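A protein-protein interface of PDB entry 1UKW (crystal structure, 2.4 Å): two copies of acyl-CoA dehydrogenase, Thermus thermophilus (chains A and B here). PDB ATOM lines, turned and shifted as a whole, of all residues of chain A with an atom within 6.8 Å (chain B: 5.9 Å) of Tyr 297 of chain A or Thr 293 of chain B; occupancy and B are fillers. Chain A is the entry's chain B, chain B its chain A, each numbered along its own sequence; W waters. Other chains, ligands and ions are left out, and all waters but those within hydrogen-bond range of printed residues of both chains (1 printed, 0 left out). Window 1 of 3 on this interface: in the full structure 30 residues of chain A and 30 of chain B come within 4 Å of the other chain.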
ATOM      1  N   ILE A 243       5.622   9.009   3.990  1.00  0.00           N
ATOM      2  CA  ILE A 243       6.305   9.571   2.831  1.00  0.00           C
ATOM      3  C   ILE A 243       7.803   9.263   2.916  1.00  0.00           C
ATOM      4  O   ILE A 243       8.423   8.898   1.922  1.00  0.00           O
ATOM      5  CB  ILE A 243       6.061  11.096   2.740  1.00  0.00           C
ATOM      6  CG1 ILE A 243       4.556  11.361   2.568  1.00  0.00           C
ATOM      7  CG2 ILE A 243       6.844  11.689   1.573  1.00  0.00           C
ATOM      8  CD1 ILE A 243       4.185  12.813   2.482  1.00  0.00           C
ATOM      9  N   ILE A 291      11.845   3.266  -9.825  1.00  0.00           N
ATOM     10  CA  ILE A 291      12.558   4.329  -9.131  1.00  0.00           C
ATOM     11  C   ILE A 291      12.049   5.729  -9.506  1.00  0.00           C
ATOM     12  O   ILE A 291      11.600   6.491  -8.651  1.00  0.00           O
ATOM     13  CB  ILE A 291      14.071   4.272  -9.450  1.00  0.00           C
ATOM     14  CG1 ILE A 291      14.676   2.989  -8.877  1.00  0.00           C
ATOM     15  CG2 ILE A 291      14.765   5.513  -8.902  1.00  0.00           C
ATOM     16  CD1 ILE A 291      16.085   2.705  -9.353  1.00  0.00           C
ATOM     17  N   GLU A 292      12.142   6.050 -10.791  1.00  0.00           N
ATOM     18  CA  GLU A 292      11.732   7.340 -11.326  1.00  0.00           C
ATOM     19  C   GLU A 292      10.279   7.690 -11.038  1.00  0.00           C
ATOM     20  O   GLU A 292       9.968   8.816 -10.655  1.00  0.00           O
ATOM     21  CB  GLU A 292      11.966   7.363 -12.840  1.00  0.00           C
ATOM     22  CG  GLU A 292      13.423   7.216 -13.249  1.00  0.00           C
ATOM     23  CD  GLU A 292      14.215   8.479 -13.020  1.00  0.00           C
ATOM     24  OE1 GLU A 292      15.367   8.380 -12.536  1.00  0.00           O
ATOM     25  OE2 GLU A 292      13.686   9.567 -13.333  1.00  0.00           O
ATOM     26  N   THR A 293       9.388   6.728 -11.243  1.00  0.00           N
ATOM     27  CA  THR A 293       7.976   6.959 -11.005  1.00  0.00           C
ATOM     28  C   THR A 293       7.683   7.045  -9.511  1.00  0.00           C
ATOM     29  O   THR A 293       6.844   7.825  -9.089  1.00  0.00           O
ATOM     30  CB  THR A 293       7.111   5.843 -11.637  1.00  0.00           C
ATOM     31  OG1 THR A 293       7.495   4.573 -11.101  1.00  0.00           O
ATOM     32  CG2 THR A 293       7.280   5.831 -13.153  1.00  0.00           C
ATOM     33  N   ALA A 294       8.381   6.252  -8.710  1.00  0.00           N
ATOM     34  CA  ALA A 294       8.152   6.273  -7.274  1.00  0.00           C
ATOM     35  C   ALA A 294       8.683   7.552  -6.634  1.00  0.00           C
ATOM     36  O   ALA A 294       8.070   8.091  -5.712  1.00  0.00           O
ATOM     37  CB  ALA A 294       8.788   5.052  -6.615  1.00  0.00           C
ATOM     38  N   ARG A 295       9.819   8.044  -7.116  1.00  0.00           N
ATOM     39  CA  ARG A 295      10.369   9.264  -6.537  1.00  0.00           C
ATOM     40  C   ARG A 295       9.473  10.454  -6.854  1.00  0.00           C
ATOM     41  O   ARG A 295       9.171  11.250  -5.971  1.00  0.00           O
ATOM     42  CB  ARG A 295      11.798   9.535  -7.038  1.00  0.00           C
ATOM     43  CG  ARG A 295      12.363  10.876  -6.552  1.00  0.00           C
ATOM     44  CD  ARG A 295      13.874  10.983  -6.717  1.00  0.00           C
ATOM     45  NE  ARG A 295      14.261  10.692  -8.083  1.00  0.00           N
ATOM     46  CZ  ARG A 295      15.066   9.701  -8.444  1.00  0.00           C
ATOM     47  NH1 ARG A 295      15.594   8.894  -7.532  1.00  0.00           N
ATOM     48  NH2 ARG A 295      15.306   9.505  -9.733  1.00  0.00           N
ATOM     49  N   MET A 296       9.039  10.568  -8.106  1.00  0.00           N
ATOM     50  CA  MET A 296       8.193  11.692  -8.484  1.00  0.00           C
ATOM     51  C   MET A 296       6.882  11.688  -7.732  1.00  0.00           C
ATOM     52  O   MET A 296       6.404  12.744  -7.321  1.00  0.00           O
ATOM     53  CB  MET A 296       7.935  11.717  -9.992  1.00  0.00           C
ATOM     54  CG  MET A 296       9.171  12.071 -10.810  1.00  0.00           C
ATOM     55  SD  MET A 296      10.060  13.531 -10.174  1.00  0.00           S
ATOM     56  CE  MET A 296      11.296  12.754  -9.192  1.00  0.00           C
ATOM     57  N   TYR A 297       6.299  10.514  -7.532  1.00  0.00           N
ATOM     58  CA  TYR A 297       5.053  10.478  -6.790  1.00  0.00           C
ATOM     59  C   TYR A 297       5.319  10.754  -5.306  1.00  0.00           C
ATOM     60  O   TYR A 297       4.450  11.259  -4.593  1.00  0.00           O
ATOM     61  CB  TYR A 297       4.325   9.139  -6.936  1.00  0.00           C
ATOM     62  CG  TYR A 297       2.877   9.303  -6.552  1.00  0.00           C
ATOM     63  CD1 TYR A 297       2.001   9.992  -7.390  1.00  0.00           C
ATOM     64  CD2 TYR A 297       2.417   8.915  -5.292  1.00  0.00           C
ATOM     65  CE1 TYR A 297       0.712  10.307  -6.983  1.00  0.00           C
ATOM     66  CE2 TYR A 297       1.123   9.229  -4.873  1.00  0.00           C
ATOM     67  CZ  TYR A 297       0.282   9.927  -5.723  1.00  0.00           C
ATOM     68  OH  TYR A 297      -0.981  10.281  -5.316  1.00  0.00           O
ATOM     69  N   THR A 298       6.520  10.423  -4.845  1.00  0.00           N
ATOM     70  CA  THR A 298       6.879  10.666  -3.456  1.00  0.00           C
ATOM     71  C   THR A 298       7.060  12.179  -3.256  1.00  0.00           C
ATOM     72  O   THR A 298       6.690  12.726  -2.215  1.00  0.00           O
ATOM     73  CB  THR A 298       8.186   9.917  -3.075  1.00  0.00           C
ATOM     74  OG1 THR A 298       7.990   8.500  -3.225  1.00  0.00           O
ATOM     75  CG2 THR A 298       8.585  10.228  -1.632  1.00  0.00           C
ATOM     76  N   TYR A 299       7.626  12.853  -4.256  1.00  0.00           N
ATOM     77  CA  TYR A 299       7.816  14.296  -4.176  1.00  0.00           C
ATOM     78  C   TYR A 299       6.451  14.979  -4.156  1.00  0.00           C
ATOM     79  O   TYR A 299       6.245  15.939  -3.422  1.00  0.00           O
ATOM     80  CB  TYR A 299       8.623  14.820  -5.377  1.00  0.00           C
ATOM     81  CG  TYR A 299      10.122  14.674  -5.256  1.00  0.00           C
ATOM     82  CD1 TYR A 299      10.714  14.351  -4.039  1.00  0.00           C
ATOM     83  CD2 TYR A 299      10.954  14.882  -6.358  1.00  0.00           C
ATOM     84  CE1 TYR A 299      12.094  14.234  -3.919  1.00  0.00           C
ATOM     85  CE2 TYR A 299      12.345  14.769  -6.248  1.00  0.00           C
ATOM     86  CZ  TYR A 299      12.903  14.442  -5.023  1.00  0.00           C
ATOM     87  OH  TYR A 299      14.272  14.302  -4.886  1.00  0.00           O
ATOM     88  N   TYR A 300       5.528  14.474  -4.971  1.00  0.00           N
ATOM     89  CA  TYR A 300       4.176  15.017  -5.056  1.00  0.00           C
ATOM     90  C   TYR A 300       3.484  14.897  -3.711  1.00  0.00           C
ATOM     91  O   TYR A 300       2.802  15.826  -3.275  1.00  0.00           O
ATOM     92  CB  TYR A 300       3.363  14.276  -6.124  1.00  0.00           C
ATOM     93  CG  TYR A 300       1.890  14.639  -6.141  1.00  0.00           C
ATOM     94  CD1 TYR A 300       0.908  13.672  -5.890  1.00  0.00           C
ATOM     95  CD2 TYR A 300       1.475  15.950  -6.387  1.00  0.00           C
ATOM     96  CE1 TYR A 300      -0.446  14.004  -5.888  1.00  0.00           C
ATOM     97  CE2 TYR A 300       0.126  16.294  -6.383  1.00  0.00           C
ATOM     98  CZ  TYR A 300      -0.827  15.321  -6.134  1.00  0.00           C
ATOM     99  OH  TYR A 300      -2.161  15.664  -6.137  1.00  0.00           O
ATOM    100  N   ALA A 301       3.662  13.751  -3.057  1.00  0.00           N
ATOM    101  CA  ALA A 301       3.067  13.518  -1.747  1.00  0.00           C
ATOM    102  C   ALA A 301       3.633  14.509  -0.726  1.00  0.00           C
ATOM    103  O   ALA A 301       2.887  15.082   0.074  1.00  0.00           O
ATOM    104  CB  ALA A 301       3.337  12.090  -1.295  1.00  0.00           C
ATOM    105  N   ALA A 302       4.953  14.699  -0.755  1.00  0.00           N
ATOM    106  CA  ALA A 302       5.618  15.627   0.158  1.00  0.00           C
ATOM    107  C   ALA A 302       5.147  17.059  -0.126  1.00  0.00           C
ATOM    108  O   ALA A 302       4.976  17.864   0.790  1.00  0.00           O
ATOM    109  CB  ALA A 302       7.134  15.527   0.002  1.00  0.00           C
ATOM    110  N   LEU A 304       2.167  17.993  -1.330  1.00  0.00           N
ATOM    111  CA  LEU A 304       0.818  18.125  -0.781  1.00  0.00           C
ATOM    112  C   LEU A 304       0.856  18.409   0.706  1.00  0.00           C
ATOM    113  O   LEU A 304       0.170  19.312   1.198  1.00  0.00           O
ATOM    114  CB  LEU A 304       0.013  16.843  -1.002  1.00  0.00           C
ATOM    115  CG  LEU A 304      -0.288  16.458  -2.445  1.00  0.00           C
ATOM    116  CD1 LEU A 304      -0.941  15.090  -2.479  1.00  0.00           C
ATOM    117  CD2 LEU A 304      -1.190  17.511  -3.074  1.00  0.00           C
ATOM    118  N   HIS A 313      -4.135   9.590   1.233  1.00  0.00           N
ATOM    119  CA  HIS A 313      -4.179   8.650   0.117  1.00  0.00           C
ATOM    120  C   HIS A 313      -2.867   8.631  -0.693  1.00  0.00           C
ATOM    121  O   HIS A 313      -2.386   7.566  -1.103  1.00  0.00           O
ATOM    122  CB  HIS A 313      -5.352   8.997  -0.808  1.00  0.00           C
ATOM    123  CG  HIS A 313      -5.123  10.227  -1.627  1.00  0.00           C
ATOM    124  ND1 HIS A 313      -4.938  11.470  -1.063  1.00  0.00           N
ATOM    125  CD2 HIS A 313      -4.959  10.390  -2.961  1.00  0.00           C
ATOM    126  CE1 HIS A 313      -4.664  12.348  -2.013  1.00  0.00           C
ATOM    127  NE2 HIS A 313      -4.669  11.717  -3.175  1.00  0.00           N
ATOM    128  N   ALA A 314      -2.294   9.813  -0.915  1.00  0.00           N
ATOM    129  CA  ALA A 314      -1.057   9.942  -1.683  1.00  0.00           C
ATOM    130  C   ALA A 314       0.157   9.287  -1.008  1.00  0.00           C
ATOM    131  O   ALA A 314       0.942   8.600  -1.664  1.00  0.00           O
ATOM    132  CB  ALA A 314      -0.773  11.409  -1.963  1.00  0.00           C
ATOM    133  N   SER A 315       0.312   9.491   0.296  1.00  0.00           N
ATOM    134  CA  SER A 315       1.449   8.902   0.997  1.00  0.00           C
ATOM    135  C   SER A 315       1.294   7.390   1.131  1.00  0.00           C
ATOM    136  O   SER A 315       2.286   6.666   1.204  1.00  0.00           O
ATOM    137  CB  SER A 315       1.621   9.537   2.387  1.00  0.00           C
ATOM    138  OG  SER A 315       0.562   9.204   3.264  1.00  0.00           O
ATOM    139  N   ALA A 316       0.050   6.924   1.172  1.00  0.00           N
ATOM    140  CA  ALA A 316      -0.230   5.500   1.283  1.00  0.00           C
ATOM    141  C   ALA A 316       0.186   4.845  -0.024  1.00  0.00           C
ATOM    142  O   ALA A 316       0.756   3.760  -0.032  1.00  0.00           O
ATOM    143  CB  ALA A 316      -1.713   5.267   1.531  1.00  0.00           C
ATOM    144  N   ILE A 317      -0.118   5.528  -1.123  1.00  0.00           N
ATOM    145  CA  ILE A 317       0.220   5.060  -2.458  1.00  0.00           C
ATOM    146  C   ILE A 317       1.736   5.073  -2.643  1.00  0.00           C
ATOM    147  O   ILE A 317       2.311   4.111  -3.155  1.00  0.00           O
ATOM    148  CB  ILE A 317      -0.427   5.956  -3.555  1.00  0.00           C
ATOM    149  CG1 ILE A 317      -1.948   5.770  -3.562  1.00  0.00           C
ATOM    150  CG2 ILE A 317       0.153   5.615  -4.923  1.00  0.00           C
ATOM    151  CD1 ILE A 317      -2.664   6.624  -4.575  1.00  0.00           C
ATOM    152  N   ALA A 318       2.378   6.159  -2.218  1.00  0.00           N
ATOM    153  CA  ALA A 318       3.822   6.287  -2.342  1.00  0.00           C
ATOM    154  C   ALA A 318       4.540   5.197  -1.557  1.00  0.00           C
ATOM    155  O   ALA A 318       5.441   4.542  -2.075  1.00  0.00           O
ATOM    156  CB  ALA A 318       4.266   7.648  -1.861  1.00  0.00           C
ATOM    157  N   LYS A 319       4.123   5.001  -0.312  1.00  0.00           N
ATOM    158  CA  LYS A 319       4.723   4.005   0.564  1.00  0.00           C
ATOM    159  C   LYS A 319       4.593   2.579   0.003  1.00  0.00           C
ATOM    160  O   LYS A 319       5.583   1.846  -0.109  1.00  0.00           O
ATOM    161  CB  LYS A 319       4.065   4.100   1.946  1.00  0.00           C
ATOM    162  CG  LYS A 319       4.789   3.394   3.068  1.00  0.00           C
ATOM    163  CD  LYS A 319       4.412   1.943   3.159  1.00  0.00           C
ATOM    164  CE  LYS A 319       4.769   1.379   4.524  1.00  0.00           C
ATOM    165  NZ  LYS A 319       4.504  -0.076   4.579  1.00  0.00           N
ATOM    166  N   TYR A 321       3.649   1.618  -3.150  1.00  0.00           N
ATOM    167  CA  TYR A 321       4.260   1.492  -4.466  1.00  0.00           C
ATOM    168  C   TYR A 321       5.791   1.418  -4.402  1.00  0.00           C
ATOM    169  O   TYR A 321       6.394   0.440  -4.856  1.00  0.00           O
ATOM    170  CB  TYR A 321       3.841   2.657  -5.373  1.00  0.00           C
ATOM    171  CG  TYR A 321       4.411   2.561  -6.777  1.00  0.00           C
ATOM    172  CD1 TYR A 321       4.003   1.554  -7.650  1.00  0.00           C
ATOM    173  CD2 TYR A 321       5.384   3.457  -7.218  1.00  0.00           C
ATOM    174  CE1 TYR A 321       4.547   1.442  -8.920  1.00  0.00           C
ATOM    175  CE2 TYR A 321       5.937   3.355  -8.485  1.00  0.00           C
ATOM    176  CZ  TYR A 321       5.514   2.347  -9.330  1.00  0.00           C
ATOM    177  OH  TYR A 321       6.055   2.246 -10.589  1.00  0.00           O
ATOM    178  N   LEU B 288      -5.807   2.957  -9.164  1.00  0.00           N
ATOM    179  CA  LEU B 288      -5.454   4.306  -8.730  1.00  0.00           C
ATOM    180  C   LEU B 288      -3.949   4.481  -8.538  1.00  0.00           C
ATOM    181  O   LEU B 288      -3.394   5.510  -8.912  1.00  0.00           O
ATOM    182  CB  LEU B 288      -6.198   4.681  -7.432  1.00  0.00           C
ATOM    183  CG  LEU B 288      -6.062   6.154  -6.996  1.00  0.00           C
ATOM    184  CD1 LEU B 288      -6.543   7.061  -8.129  1.00  0.00           C
ATOM    185  CD2 LEU B 288      -6.853   6.425  -5.723  1.00  0.00           C
ATOM    186  N   ILE B 289      -3.291   3.484  -7.952  1.00  0.00           N
ATOM    187  CA  ILE B 289      -1.849   3.553  -7.754  1.00  0.00           C
ATOM    188  C   ILE B 289      -1.192   3.776  -9.111  1.00  0.00           C
ATOM    189  O   ILE B 289      -0.281   4.581  -9.244  1.00  0.00           O
ATOM    190  CB  ILE B 289      -1.294   2.248  -7.136  1.00  0.00           C
ATOM    191  CG1 ILE B 289      -1.791   2.103  -5.694  1.00  0.00           C
ATOM    192  CG2 ILE B 289       0.233   2.252  -7.184  1.00  0.00           C
ATOM    193  CD1 ILE B 289      -1.305   0.842  -4.994  1.00  0.00           C
ATOM    194  N   GLY B 290      -1.674   3.062 -10.119  1.00  0.00           N
ATOM    195  CA  GLY B 290      -1.126   3.211 -11.454  1.00  0.00           C
ATOM    196  C   GLY B 290      -1.440   4.570 -12.055  1.00  0.00           C
ATOM    197  O   GLY B 290      -0.561   5.215 -12.620  1.00  0.00           O
ATOM    198  N   ILE B 291      -2.692   5.007 -11.932  1.00  0.00           N
ATOM    199  CA  ILE B 291      -3.129   6.296 -12.464  1.00  0.00           C
ATOM    200  C   ILE B 291      -2.351   7.468 -11.877  1.00  0.00           C
ATOM    201  O   ILE B 291      -1.840   8.302 -12.608  1.00  0.00           O
ATOM    202  CB  ILE B 291      -4.630   6.522 -12.185  1.00  0.00           C
ATOM    203  CG1 ILE B 291      -5.456   5.469 -12.922  1.00  0.00           C
ATOM    204  CG2 ILE B 291      -5.041   7.931 -12.597  1.00  0.00           C
ATOM    205  CD1 ILE B 291      -6.902   5.462 -12.522  1.00  0.00           C
ATOM    206  N   GLU B 292      -2.272   7.519 -10.552  1.00  0.00           N
ATOM    207  CA  GLU B 292      -1.577   8.581  -9.827  1.00  0.00           C
ATOM    208  C   GLU B 292      -0.084   8.681 -10.098  1.00  0.00           C
ATOM    209  O   GLU B 292       0.433   9.756 -10.398  1.00  0.00           O
ATOM    210  CB  GLU B 292      -1.794   8.403  -8.322  1.00  0.00           C
ATOM    211  CG  GLU B 292      -3.228   8.628  -7.905  1.00  0.00           C
ATOM    212  CD  GLU B 292      -3.622  10.090  -7.959  1.00  0.00           C
ATOM    213  OE1 GLU B 292      -4.791  10.366  -8.301  1.00  0.00           O
ATOM    214  OE2 GLU B 292      -2.769  10.956  -7.650  1.00  0.00           O
ATOM    215  N   THR B 293       0.608   7.560  -9.977  1.00  0.00           N
ATOM    216  CA  THR B 293       2.042   7.536 -10.201  1.00  0.00           C
ATOM    217  C   THR B 293       2.370   7.787 -11.659  1.00  0.00           C
ATOM    218  O   THR B 293       3.352   8.445 -11.969  1.00  0.00           O
ATOM    219  CB  THR B 293       2.650   6.192  -9.768  1.00  0.00           C
ATOM    220  OG1 THR B 293       2.037   5.133 -10.509  1.00  0.00           O
ATOM    221  CG2 THR B 293       2.432   5.965  -8.274  1.00  0.00           C
ATOM    222  N   ALA B 294       1.545   7.264 -12.556  1.00  0.00           N
ATOM    223  CA  ALA B 294       1.779   7.463 -13.977  1.00  0.00           C
ATOM    224  C   ALA B 294       1.519   8.912 -14.371  1.00  0.00           C
ATOM    225  O   ALA B 294       2.272   9.477 -15.151  1.00  0.00           O
ATOM    226  CB  ALA B 294       0.898   6.542 -14.797  1.00  0.00           C
ATOM    227  N   ARG B 295       0.465   9.522 -13.830  1.00  0.00           N
ATOM    228  CA  ARG B 295       0.163  10.908 -14.179  1.00  0.00           C
ATOM    229  C   ARG B 295       1.259  11.882 -13.738  1.00  0.00           C
ATOM    230  O   ARG B 295       1.689  12.726 -14.525  1.00  0.00           O
ATOM    231  CB  ARG B 295      -1.186  11.341 -13.599  1.00  0.00           C
ATOM    232  CG  ARG B 295      -1.598  12.752 -13.994  1.00  0.00           C
ATOM    233  CD  ARG B 295      -3.109  12.922 -13.890  1.00  0.00           C
ATOM    234  NE  ARG B 295      -3.556  12.493 -12.578  1.00  0.00           N
ATOM    235  CZ  ARG B 295      -4.674  11.825 -12.345  1.00  0.00           C
ATOM    236  NH1 ARG B 295      -5.485  11.511 -13.346  1.00  0.00           N
ATOM    237  NH2 ARG B 295      -4.953  11.441 -11.107  1.00  0.00           N
ATOM    238  N   MET B 296       1.720  11.763 -12.494  1.00  0.00           N
ATOM    239  CA  MET B 296       2.768  12.654 -12.008  1.00  0.00           C
ATOM    240  C   MET B 296       4.046  12.504 -12.819  1.00  0.00           C
ATOM    241  O   MET B 296       4.711  13.502 -13.110  1.00  0.00           O
ATOM    242  CB  MET B 296       3.062  12.422 -10.517  1.00  0.00           C
ATOM    243  CG  MET B 296       1.864  12.692  -9.587  1.00  0.00           C
ATOM    244  SD  MET B 296       1.088  14.353  -9.766  1.00  0.00           S
ATOM    245  CE  MET B 296       0.026  14.078 -11.221  1.00  0.00           C
ATOM    246  N   TYR B 297       4.395  11.278 -13.208  1.00  0.00           N
ATOM    247  CA  TYR B 297       5.616  11.113 -13.988  1.00  0.00           C
ATOM    248  C   TYR B 297       5.443  11.659 -15.399  1.00  0.00           C
ATOM    249  O   TYR B 297       6.403  12.116 -16.010  1.00  0.00           O
ATOM    250  CB  TYR B 297       6.073   9.655 -14.062  1.00  0.00           C
ATOM    251  CG  TYR B 297       7.534   9.573 -14.439  1.00  0.00           C
ATOM    252  CD1 TYR B 297       8.530   9.845 -13.493  1.00  0.00           C
ATOM    253  CD2 TYR B 297       7.925   9.328 -15.760  1.00  0.00           C
ATOM    254  CE1 TYR B 297       9.881   9.885 -13.849  1.00  0.00           C
ATOM    255  CE2 TYR B 297       9.277   9.364 -16.132  1.00  0.00           C
ATOM    256  CZ  TYR B 297      10.249   9.646 -15.173  1.00  0.00           C
ATOM    257  OH  TYR B 297      11.576   9.716 -15.536  1.00  0.00           O
ATOM    258  N   THR B 298       4.223  11.605 -15.921  1.00  0.00           N
ATOM    259  CA  THR B 298       3.957  12.145 -17.250  1.00  0.00           C
ATOM    260  C   THR B 298       4.075  13.667 -17.142  1.00  0.00           C
ATOM    261  O   THR B 298       4.621  14.320 -18.032  1.00  0.00           O
ATOM    262  CB  THR B 298       2.550  11.779 -17.751  1.00  0.00           C
ATOM    263  OG1 THR B 298       2.450  10.359 -17.885  1.00  0.00           O
ATOM    264  CG2 THR B 298       2.283  12.425 -19.111  1.00  0.00           C
ATOM    265  N   TYR B 321       5.326   2.773 -19.075  1.00  0.00           N
ATOM    266  CA  TYR B 321       4.652   2.523 -17.810  1.00  0.00           C
ATOM    267  C   TYR B 321       3.146   2.780 -17.842  1.00  0.00           C
ATOM    268  O   TYR B 321       2.358   1.910 -17.479  1.00  0.00           O
ATOM    269  CB  TYR B 321       5.296   3.367 -16.712  1.00  0.00           C
ATOM    270  CG  TYR B 321       4.694   3.158 -15.345  1.00  0.00           C
ATOM    271  CD1 TYR B 321       4.846   1.946 -14.673  1.00  0.00           C
ATOM    272  CD2 TYR B 321       3.971   4.174 -14.724  1.00  0.00           C
ATOM    273  CE1 TYR B 321       4.293   1.751 -13.413  1.00  0.00           C
ATOM    274  CE2 TYR B 321       3.417   3.994 -13.470  1.00  0.00           C
ATOM    275  CZ  TYR B 321       3.580   2.784 -12.817  1.00  0.00           C
ATOM    276  OH  TYR B 321       3.039   2.613 -11.570  1.00  0.00           O
HETATM  277  O   HOH W   1       5.403   9.828 -10.402  1.00  0.00           O
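The side-chain hydroxyl of Thr 293 of chain B lies within hydrogen-bond range of the backbone carbonyl oxygen of Ile 289 of chain B (2.7 Å). NH2 of Arg 295 of chain A lies within salt-bridge range of OE1 of Glu 292 of chain A, at 3.0 Å. OG1 of Thr 293 of chain A is in hydrogen-bond range of OH of Tyr 321 of chain A. The guanidinium group (NH2) of Arg 295 of chain B lies within salt-bridge range of the side-chain carboxylate (OE1) of Glu 292 of chain B, at 3.0 Å. The side-chain hydroxyl (OH) of Tyr 321 of chain B lies within hydrogen-bond range of the side-chain hydroxyl (OG1) of Thr 293 of chain B (2.9 Å). OG1 of Thr 293 of chain B is in hydrogen-bond range of O of Gly 290 of chain B (3.3 Å).
Water W1 lies within hydrogen-bond range of the backbone carbonyl oxygen of Thr 293 of chain A (2.8 Å), the backbone carbonyl oxygen of Thr 293 of chain B (2.9 Å), the backbone NH of Tyr 297 of chain A (3.1 Å) and the backbone NH of Tyr 297 of chain B (3.3 Å).
Tyr 297 of chain A touches just these residues of chain B: Glu 292 (3.0 Å), Thr 293 (3.7 Å) and Met 296 (3.5 Å). Of the printed residues of chain A, Thr 293 of chain B touches Tyr 297 (3.7 Å). Printed residues of chain B within 4 Å of Ile 317 of chain A: Glu 292 (3.9 Å). Printed residues of chain A within 4 Å of Ile 289 of chain B: Tyr 321 (3.9 Å). Printed residues of chain A within 4 Å of Glu 292 of chain B: Tyr 297 (3.0 Å) and Ile 317 (3.9 Å). The nearest printed residue of chain A that does not touch Thr 293 of chain B is Tyr 321 of chain A (4.01 Å). The nearest printed residue of chain B that does not touch Met 296 of chain A is Met 296 of chain B (4.6 Å).
Thr 293 of chain A touches Tyr 297 of chain B. Met 296 of chain A touches Tyr 297 of chain B. CA of Thr 293 of chain B touches CD1 of Tyr 297 of chain A (3.7 Å). Tyr 297 of chain A touches Met 296 of chain B. Met 296 of chain B touches Tyr 300 of chain A. Ile 317 of chain A touches Glu 292 of chain B (CD1 to CG, 3.9 Å). CD1 of Tyr 321 of chain A touches CG2 of Ile 289 of chain B, 3.9 Å away.
Glu 292 of chain A touches Tyr 297 of chain B, and with the chains exchanged Tyr 297 of chain A touches Glu 292 of chain B. Thr 293 of chain A touches Tyr 297 of chain B, and with the chains exchanged Tyr 297 of chain A touches Thr 293 of chain B. Met 296 of chain A touches Tyr 297 of chain B, and with the chains exchanged Tyr 297 of chain A touches Met 296 of chain B. Tyr 321 of chain A touches its own counterpart, Tyr 321 of chain B. 9 positions are printed for both chains. Of the 10 pairs that touch across the chains among the printed residues, 7 have their exchanged pair printed and touching as well.
Of the 22 printed residues of chain A, 7 touch a printed residue of chain B. Along chain A the printed residues that touch a printed residue of chain B span positions 292 to 321. Of the 12 printed residues of chain B, 6 touch a printed residue of chain A. Among the printed residues, 10 pairs touch across the chains. Among the printed residues, no Asp or Glu carboxylate lies within 4 Å of a Lys or Arg side-chain nitrogen of the other chain.
The side-chain carboxylate (OE2) of Glu 292 of chain A sits at hydrogen-bond distance from the side-chain hydroxyl (OH) of Tyr 297 of chain B (3.1 Å). The side-chain carboxylate (OE2) of Glu 292 of chain B is in hydrogen-bond range of the side-chain hydroxyl (OH) of Tyr 297 of chain A (3.0 Å). The side-chain hydroxyl (OH) of Tyr 321 of chain B is in hydrogen-bond range of the side-chain hydroxyl (OH) of Tyr 321 of chain A (3.2 Å).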
